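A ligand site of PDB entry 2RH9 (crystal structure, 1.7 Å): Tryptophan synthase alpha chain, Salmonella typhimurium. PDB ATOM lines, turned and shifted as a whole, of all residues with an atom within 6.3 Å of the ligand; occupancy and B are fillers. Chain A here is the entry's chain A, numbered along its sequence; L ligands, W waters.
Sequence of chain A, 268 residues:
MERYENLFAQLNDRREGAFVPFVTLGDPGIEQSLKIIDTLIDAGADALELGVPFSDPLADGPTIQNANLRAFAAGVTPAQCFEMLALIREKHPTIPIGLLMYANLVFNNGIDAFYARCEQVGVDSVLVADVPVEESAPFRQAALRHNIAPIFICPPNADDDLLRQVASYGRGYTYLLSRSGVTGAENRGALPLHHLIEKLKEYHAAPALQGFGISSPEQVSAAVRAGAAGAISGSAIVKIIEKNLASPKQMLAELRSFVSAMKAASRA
Water W1 lies within hydrogen-bond range of an oxygen (O2) of the ligand, the backbone NH (N) of Ala 236, the backbone carbonyl oxygen (O) of Ile 214 and the side-chain hydroxyl (OG) of Ser 233.
The backbone NH (N) of Phe 22 lies within hydrogen-bond range of the backbone carbonyl oxygen (O) of Ser 233 (2.9 Å). OH of Tyr 102 lies within hydrogen-bond range of OD1 of Asp 60, at 2.5 Å. The backbone NH (N) of Ala 59 is in hydrogen-bond range of the side-chain hydroxyl (OH) of Tyr 102 (3.0 Å). The side-chain hydroxyl of Ser 233 lies within hydrogen-bond range of the backbone carbonyl oxygen of Ile 214, 2.7 Å away.
Phe 22 touches the ligand (CE2 to C8, 3.7 Å). Ala 59 touches the ligand (CB to C9, 3.9 Å). Ile 64 touches the ligand (CG1 to O5, 3.9 Å). Leu 100 touches the ligand (CG to C6, 3.6 Å). Ala 129 touches the ligand. CD1 of Ile 153 touches C10 of the ligand, at 3.6 Å. CA of Phe 212 touches O3 of the ligand (3.5 Å). Ile 232 touches the ligand (CG2 to O6, 3.9 Å). C of Ser 233 touches O2 of the ligand (3.9 Å). 14 residues have an atom within 4 Å of the ligand: Phe 22, Ala 59, Asp 60, Ile 64, Leu 100, Ala 129, Ile 153, Tyr 175, Phe 212, Gly 213, Ile 232, Ser 233, Gly 234 and Ser 235. The nearest printed residue that does not touch the ligand is Tyr 102 (4.1 Å).
The backbone NH (N) of Ser 235 sits at hydrogen-bond distance from an oxygen (O1) of the ligand (2.8 Å). The side-chain hydroxyl (OG) of Ser 235 lies within hydrogen-bond range of an oxygen (O1) of the ligand, 2.7 Å away. An oxygen (O6) of the ligand sits at hydrogen-bond distance from the side-chain hydroxyl (OH) of Tyr 175 (2.7 Å). The backbone NH of Gly 234 is in hydrogen-bond range of an oxygen (O2) of the ligand, at 2.9 Å. N of Gly 213 sits at hydrogen-bond distance from O3 of the ligand, 2.8 Å away. The side-chain carboxylate of Asp 60 is in hydrogen-bond range of a nitrogen (N1) of the ligand, 3.1 Å away.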
ATOM      1  N   PHE A  22       4.811 -15.267 -13.858  1.00  0.00           N
ATOM      2  CA  PHE A  22       5.357 -16.483 -13.260  1.00  0.00           C
ATOM      3  C   PHE A  22       6.502 -16.106 -12.317  1.00  0.00           C
ATOM      4  O   PHE A  22       7.376 -15.329 -12.703  1.00  0.00           O
ATOM      5  CB  PHE A  22       5.931 -17.454 -14.308  1.00  0.00           C
ATOM      6  CG  PHE A  22       6.791 -18.547 -13.707  1.00  0.00           C
ATOM      7  CD1 PHE A  22       8.123 -18.323 -13.381  1.00  0.00           C
ATOM      8  CD2 PHE A  22       6.251 -19.792 -13.420  1.00  0.00           C
ATOM      9  CE1 PHE A  22       8.883 -19.304 -12.811  1.00  0.00           C
ATOM     10  CE2 PHE A  22       7.028 -20.788 -12.858  1.00  0.00           C
ATOM     11  CZ  PHE A  22       8.338 -20.546 -12.540  1.00  0.00           C
ATOM     12  N   GLU A  49       1.193 -17.858 -12.122  1.00  0.00           N
ATOM     13  CA  GLU A  49       1.801 -19.167 -12.355  1.00  0.00           C
ATOM     14  C   GLU A  49       2.983 -19.262 -11.384  1.00  0.00           C
ATOM     15  O   GLU A  49       3.825 -18.366 -11.326  1.00  0.00           O
ATOM     16  CB  GLU A  49       2.261 -19.309 -13.806  1.00  0.00           C
ATOM     17  CG  GLU A  49       2.515 -20.755 -14.215  1.00  0.00           C
ATOM     18  CD  GLU A  49       1.260 -21.529 -14.606  1.00  0.00           C
ATOM     19  OE1 GLU A  49       1.445 -22.707 -14.983  1.00  0.00           O
ATOM     20  OE2 GLU A  49       0.117 -21.011 -14.552  1.00  0.00           O
ATOM     21  N   ALA A  59      12.926 -28.303 -18.432  1.00  0.00           N
ATOM     22  CA  ALA A  59      12.218 -27.352 -19.317  1.00  0.00           C
ATOM     23  C   ALA A  59      12.428 -25.889 -18.926  1.00  0.00           C
ATOM     24  O   ALA A  59      11.924 -24.995 -19.592  1.00  0.00           O
ATOM     25  CB  ALA A  59      10.744 -27.671 -19.379  1.00  0.00           C
ATOM     26  N   ASP A  60      13.166 -25.635 -17.840  1.00  0.00           N
ATOM     27  CA  ASP A  60      13.424 -24.265 -17.380  1.00  0.00           C
ATOM     28  C   ASP A  60      14.706 -23.727 -18.057  1.00  0.00           C
ATOM     29  O   ASP A  60      15.739 -24.408 -18.076  1.00  0.00           O
ATOM     30  CB  ASP A  60      13.631 -24.202 -15.844  1.00  0.00           C
ATOM     31  CG  ASP A  60      12.410 -24.673 -15.018  1.00  0.00           C
ATOM     32  OD1 ASP A  60      11.343 -25.003 -15.538  1.00  0.00           O
ATOM     33  OD2 ASP A  60      12.542 -24.724 -13.763  1.00  0.00           O
ATOM     34  N   GLY A  61      14.658 -22.492 -18.579  1.00  0.00           N
ATOM     35  CA  GLY A  61      15.865 -21.770 -19.026  1.00  0.00           C
ATOM     36  C   GLY A  61      16.737 -21.288 -17.869  1.00  0.00           C
ATOM     37  O   GLY A  61      16.332 -21.421 -16.710  1.00  0.00           O
ATOM     38  N   ILE A  64      15.229 -19.123 -14.925  1.00  0.00           N
ATOM     39  CA  ILE A  64      14.394 -19.912 -14.026  1.00  0.00           C
ATOM     40  C   ILE A  64      15.278 -20.905 -13.246  1.00  0.00           C
ATOM     41  O   ILE A  64      15.109 -21.068 -12.046  1.00  0.00           O
ATOM     42  CB  ILE A  64      13.233 -20.613 -14.810  1.00  0.00           C
ATOM     43  CG1 ILE A  64      12.415 -19.603 -15.626  1.00  0.00           C
ATOM     44  CG2 ILE A  64      12.300 -21.344 -13.846  1.00  0.00           C
ATOM     45  CD1 ILE A  64      12.072 -18.324 -14.895  1.00  0.00           C
ATOM     46  N   LEU A 100       3.404 -24.666 -11.742  1.00  0.00           N
ATOM     47  CA  LEU A 100       4.268 -25.238 -12.756  1.00  0.00           C
ATOM     48  C   LEU A 100       5.091 -26.280 -12.020  1.00  0.00           C
ATOM     49  O   LEU A 100       5.923 -25.969 -11.145  1.00  0.00           O
ATOM     50  CB  LEU A 100       5.147 -24.167 -13.407  1.00  0.00           C
ATOM     51  CG  LEU A 100       6.022 -24.604 -14.601  1.00  0.00           C
ATOM     52  CD1 LEU A 100       7.114 -25.585 -14.187  1.00  0.00           C
ATOM     53  CD2 LEU A 100       5.216 -25.176 -15.768  1.00  0.00           C
ATOM     54  N   TYR A 102       7.076 -30.329 -11.981  1.00  0.00           N
ATOM     55  CA  TYR A 102       7.739 -31.429 -12.648  1.00  0.00           C
ATOM     56  C   TYR A 102       7.127 -32.718 -12.111  1.00  0.00           C
ATOM     57  O   TYR A 102       6.714 -32.807 -10.949  1.00  0.00           O
ATOM     58  CB  TYR A 102       9.249 -31.342 -12.448  1.00  0.00           C
ATOM     59  CG  TYR A 102       9.824 -30.277 -13.388  1.00  0.00           C
ATOM     60  CD1 TYR A 102      10.224 -30.607 -14.669  1.00  0.00           C
ATOM     61  CD2 TYR A 102       9.888 -28.944 -13.012  1.00  0.00           C
ATOM     62  CE1 TYR A 102      10.696 -29.637 -15.559  1.00  0.00           C
ATOM     63  CE2 TYR A 102      10.375 -27.965 -13.887  1.00  0.00           C
ATOM     64  CZ  TYR A 102      10.772 -28.329 -15.160  1.00  0.00           C
ATOM     65  OH  TYR A 102      11.253 -27.401 -16.053  1.00  0.00           O
ATOM     66  N   LEU A 127       0.208 -27.351 -14.410  1.00  0.00           N
ATOM     67  CA  LEU A 127       0.916 -27.676 -15.631  1.00  0.00           C
ATOM     68  C   LEU A 127       2.117 -28.544 -15.212  1.00  0.00           C
ATOM     69  O   LEU A 127       2.998 -28.096 -14.473  1.00  0.00           O
ATOM     70  CB  LEU A 127       1.367 -26.375 -16.311  1.00  0.00           C
ATOM     71  CG  LEU A 127       1.744 -26.473 -17.802  1.00  0.00           C
ATOM     72  CD1 LEU A 127       2.227 -25.139 -18.359  1.00  0.00           C
ATOM     73  CD2 LEU A 127       2.774 -27.532 -18.060  1.00  0.00           C
ATOM     74  N   ALA A 129       5.266 -29.999 -16.514  1.00  0.00           N
ATOM     75  CA  ALA A 129       6.082 -29.586 -17.677  1.00  0.00           C
ATOM     76  C   ALA A 129       6.619 -30.784 -18.490  1.00  0.00           C
ATOM     77  O   ALA A 129       6.776 -30.670 -19.725  1.00  0.00           O
ATOM     78  CB  ALA A 129       7.210 -28.721 -17.213  1.00  0.00           C
ATOM     79  N   ILE A 153       0.517 -27.637 -22.777  1.00  0.00           N
ATOM     80  CA  ILE A 153       1.301 -26.776 -23.637  1.00  0.00           C
ATOM     81  C   ILE A 153       0.990 -27.117 -25.070  1.00  0.00           C
ATOM     82  O   ILE A 153       0.984 -28.300 -25.472  1.00  0.00           O
ATOM     83  CB  ILE A 153       2.809 -26.915 -23.366  1.00  0.00           C
ATOM     84  CG1 ILE A 153       3.158 -26.233 -22.040  1.00  0.00           C
ATOM     85  CG2 ILE A 153       3.641 -26.312 -24.500  1.00  0.00           C
ATOM     86  CD1 ILE A 153       4.559 -26.464 -21.559  1.00  0.00           C
ATOM     87  N   TYR A 175      -1.852 -23.395 -22.614  1.00  0.00           N
ATOM     88  CA  TYR A 175      -0.559 -22.712 -22.623  1.00  0.00           C
ATOM     89  C   TYR A 175      -0.047 -22.720 -24.046  1.00  0.00           C
ATOM     90  O   TYR A 175       0.405 -23.743 -24.547  1.00  0.00           O
ATOM     91  CB  TYR A 175       0.456 -23.365 -21.676  1.00  0.00           C
ATOM     92  CG  TYR A 175       1.674 -22.513 -21.340  1.00  0.00           C
ATOM     93  CD1 TYR A 175       2.599 -22.158 -22.315  1.00  0.00           C
ATOM     94  CD2 TYR A 175       1.924 -22.127 -20.039  1.00  0.00           C
ATOM     95  CE1 TYR A 175       3.718 -21.421 -22.020  1.00  0.00           C
ATOM     96  CE2 TYR A 175       3.066 -21.354 -19.735  1.00  0.00           C
ATOM     97  CZ  TYR A 175       3.946 -21.001 -20.732  1.00  0.00           C
ATOM     98  OH  TYR A 175       5.075 -20.256 -20.452  1.00  0.00           O
ATOM     99  N   LEU A 177       2.595 -21.926 -26.520  1.00  0.00           N
ATOM    100  CA  LEU A 177       4.021 -21.635 -26.563  1.00  0.00           C
ATOM    101  C   LEU A 177       4.313 -20.697 -27.742  1.00  0.00           C
ATOM    102  O   LEU A 177       3.738 -20.846 -28.841  1.00  0.00           O
ATOM    103  CB  LEU A 177       4.812 -22.942 -26.683  1.00  0.00           C
ATOM    104  CG  LEU A 177       6.254 -22.997 -26.201  1.00  0.00           C
ATOM    105  CD1 LEU A 177       6.360 -22.544 -24.758  1.00  0.00           C
ATOM    106  CD2 LEU A 177       6.781 -24.435 -26.372  1.00  0.00           C
ATOM    107  N   GLY A 211       2.806 -17.809 -23.905  1.00  0.00           N
ATOM    108  CA  GLY A 211       3.974 -17.793 -23.024  1.00  0.00           C
ATOM    109  C   GLY A 211       5.261 -18.155 -23.757  1.00  0.00           C
ATOM    110  O   GLY A 211       5.223 -18.784 -24.820  1.00  0.00           O
ATOM    111  N   PHE A 212       6.382 -17.794 -23.139  1.00  0.00           N
ATOM    112  CA  PHE A 212       7.741 -17.896 -23.710  1.00  0.00           C
ATOM    113  C   PHE A 212       8.173 -16.597 -24.378  1.00  0.00           C
ATOM    114  O   PHE A 212       7.609 -16.203 -25.417  1.00  0.00           O
ATOM    115  CB  PHE A 212       7.913 -19.100 -24.681  1.00  0.00           C
ATOM    116  N   GLY A 213       9.143 -15.933 -23.758  1.00  0.00           N
ATOM    117  CA  GLY A 213       9.767 -14.738 -24.307  1.00  0.00           C
ATOM    118  C   GLY A 213       8.964 -13.447 -24.259  1.00  0.00           C
ATOM    119  O   GLY A 213       9.336 -12.480 -24.914  1.00  0.00           O
ATOM    120  N   ILE A 214       7.858 -13.417 -23.493  1.00  0.00           N
ATOM    121  CA  ILE A 214       7.033 -12.224 -23.335  1.00  0.00           C
ATOM    122  C   ILE A 214       7.681 -11.303 -22.297  1.00  0.00           C
ATOM    123  O   ILE A 214       7.627 -11.584 -21.084  1.00  0.00           O
ATOM    124  CB  ILE A 214       5.587 -12.559 -22.827  1.00  0.00           C
ATOM    125  CG1 ILE A 214       4.874 -13.552 -23.763  1.00  0.00           C
ATOM    126  CG2 ILE A 214       4.749 -11.296 -22.630  1.00  0.00           C
ATOM    127  CD1 ILE A 214       4.401 -12.980 -25.075  1.00  0.00           C
ATOM    128  N   SER A 215       8.286 -10.192 -22.755  1.00  0.00           N
ATOM    129  CA  SER A 215       8.995  -9.297 -21.832  1.00  0.00           C
ATOM    130  C   SER A 215       8.679  -7.809 -21.991  1.00  0.00           C
ATOM    131  O   SER A 215       9.264  -6.992 -21.285  1.00  0.00           O
ATOM    132  CB  SER A 215      10.500  -9.489 -21.985  1.00  0.00           C
ATOM    133  OG  SER A 215      10.917  -9.136 -23.293  1.00  0.00           O
ATOM    134  N   ILE A 232       1.541 -14.756 -20.533  1.00  0.00           N
ATOM    135  CA  ILE A 232       2.301 -15.155 -19.361  1.00  0.00           C
ATOM    136  C   ILE A 232       3.750 -14.645 -19.476  1.00  0.00           C
ATOM    137  O   ILE A 232       4.372 -14.764 -20.535  1.00  0.00           O
ATOM    138  CB  ILE A 232       2.326 -16.702 -19.209  1.00  0.00           C
ATOM    139  CG1 ILE A 232       0.947 -17.225 -18.775  1.00  0.00           C
ATOM    140  CG2 ILE A 232       3.422 -17.162 -18.222  1.00  0.00           C
ATOM    141  CD1 ILE A 232       0.679 -18.670 -19.254  1.00  0.00           C
ATOM    142  N   SER A 233       4.300 -14.096 -18.407  1.00  0.00           N
ATOM    143  CA  SER A 233       5.685 -13.661 -18.434  1.00  0.00           C
ATOM    144  C   SER A 233       6.426 -14.155 -17.190  1.00  0.00           C
ATOM    145  O   SER A 233       5.986 -13.893 -16.084  1.00  0.00           O
ATOM    146  CB  SER A 233       5.758 -12.133 -18.534  1.00  0.00           C
ATOM    147  OG  SER A 233       7.105 -11.690 -18.437  1.00  0.00           O
ATOM    148  N   GLY A 234       7.534 -14.862 -17.396  1.00  0.00           N
ATOM    149  CA  GLY A 234       8.343 -15.397 -16.286  1.00  0.00           C
ATOM    150  C   GLY A 234       9.738 -14.838 -16.186  1.00  0.00           C
ATOM    151  O   GLY A 234      10.039 -14.072 -15.274  1.00  0.00           O
ATOM    152  N   SER A 235      10.604 -15.231 -17.119  1.00  0.00           N
ATOM    153  CA  SER A 235      11.998 -14.787 -17.080  1.00  0.00           C
ATOM    154  C   SER A 235      12.127 -13.279 -16.877  1.00  0.00           C
ATOM    155  O   SER A 235      12.918 -12.823 -16.053  1.00  0.00           O
ATOM    156  CB  SER A 235      12.747 -15.229 -18.331  1.00  0.00           C
ATOM    157  OG  SER A 235      12.875 -16.630 -18.338  1.00  0.00           O
ATOM    158  N   ALA A 236      11.315 -12.497 -17.576  1.00  0.00           N
ATOM    159  CA  ALA A 236      11.347 -11.045 -17.436  1.00  0.00           C
ATOM    160  C   ALA A 236      11.126 -10.616 -16.007  1.00  0.00           C
ATOM    161  O   ALA A 236      11.835  -9.729 -15.497  1.00  0.00           O
ATOM    162  CB  ALA A 236      10.307 -10.404 -18.340  1.00  0.00           C
HETATM  163  C1  LIG L   1       7.514 -18.369 -19.087  1.00  0.00           C
HETATM  164  P1  LIG L   1       9.451 -16.931 -20.115  1.00  0.00           P
HETATM  165  O1  LIG L   1      10.297 -17.303 -18.906  1.00  0.00           O
HETATM  166  O2  LIG L   1       8.685 -15.620 -19.947  1.00  0.00           O
HETATM  167  O3  LIG L   1      10.225 -16.998 -21.411  1.00  0.00           O
HETATM  168  O4  LIG L   1       8.326 -18.087 -20.226  1.00  0.00           O
HETATM  169  C2  LIG L   1       7.973 -19.703 -18.534  1.00  0.00           C
HETATM  170  O5  LIG L   1       9.318 -19.544 -18.056  1.00  0.00           O
HETATM  171  C3  LIG L   1       7.098 -20.244 -17.401  1.00  0.00           C
HETATM  172  O6  LIG L   1       5.723 -20.259 -17.787  1.00  0.00           O
HETATM  173  C4  LIG L   1       7.665 -21.584 -17.123  1.00  0.00           C
HETATM  174  C5  LIG L   1       7.474 -22.782 -17.946  1.00  0.00           C
HETATM  175  C6  LIG L   1       8.328 -23.771 -17.255  1.00  0.00           C
HETATM  176  C7  LIG L   1       6.712 -23.110 -19.048  1.00  0.00           C
HETATM  177  C8  LIG L   1       8.577 -21.838 -16.101  1.00  0.00           C
HETATM  178  N1  LIG L   1       8.933 -23.160 -16.206  1.00  0.00           N
HETATM  179  C9  LIG L   1       8.355 -25.056 -17.781  1.00  0.00           C
HETATM  180  C10 LIG L   1       6.776 -24.410 -19.527  1.00  0.00           C
HETATM  181  C11 LIG L   1       7.572 -25.370 -18.905  1.00  0.00           C
HETATM  182  O   HOH W   1       9.686 -13.203 -19.846  1.00  0.00           O
HETATM  183  O   HOH W   2       6.748 -15.423 -21.682  1.00  0.00           O
HETATM  184  O   HOH W   3      10.931 -21.716 -18.681  1.00  0.00           O
HETATM  185  O   HOH W   4      12.795 -15.810 -22.185  1.00  0.00           O
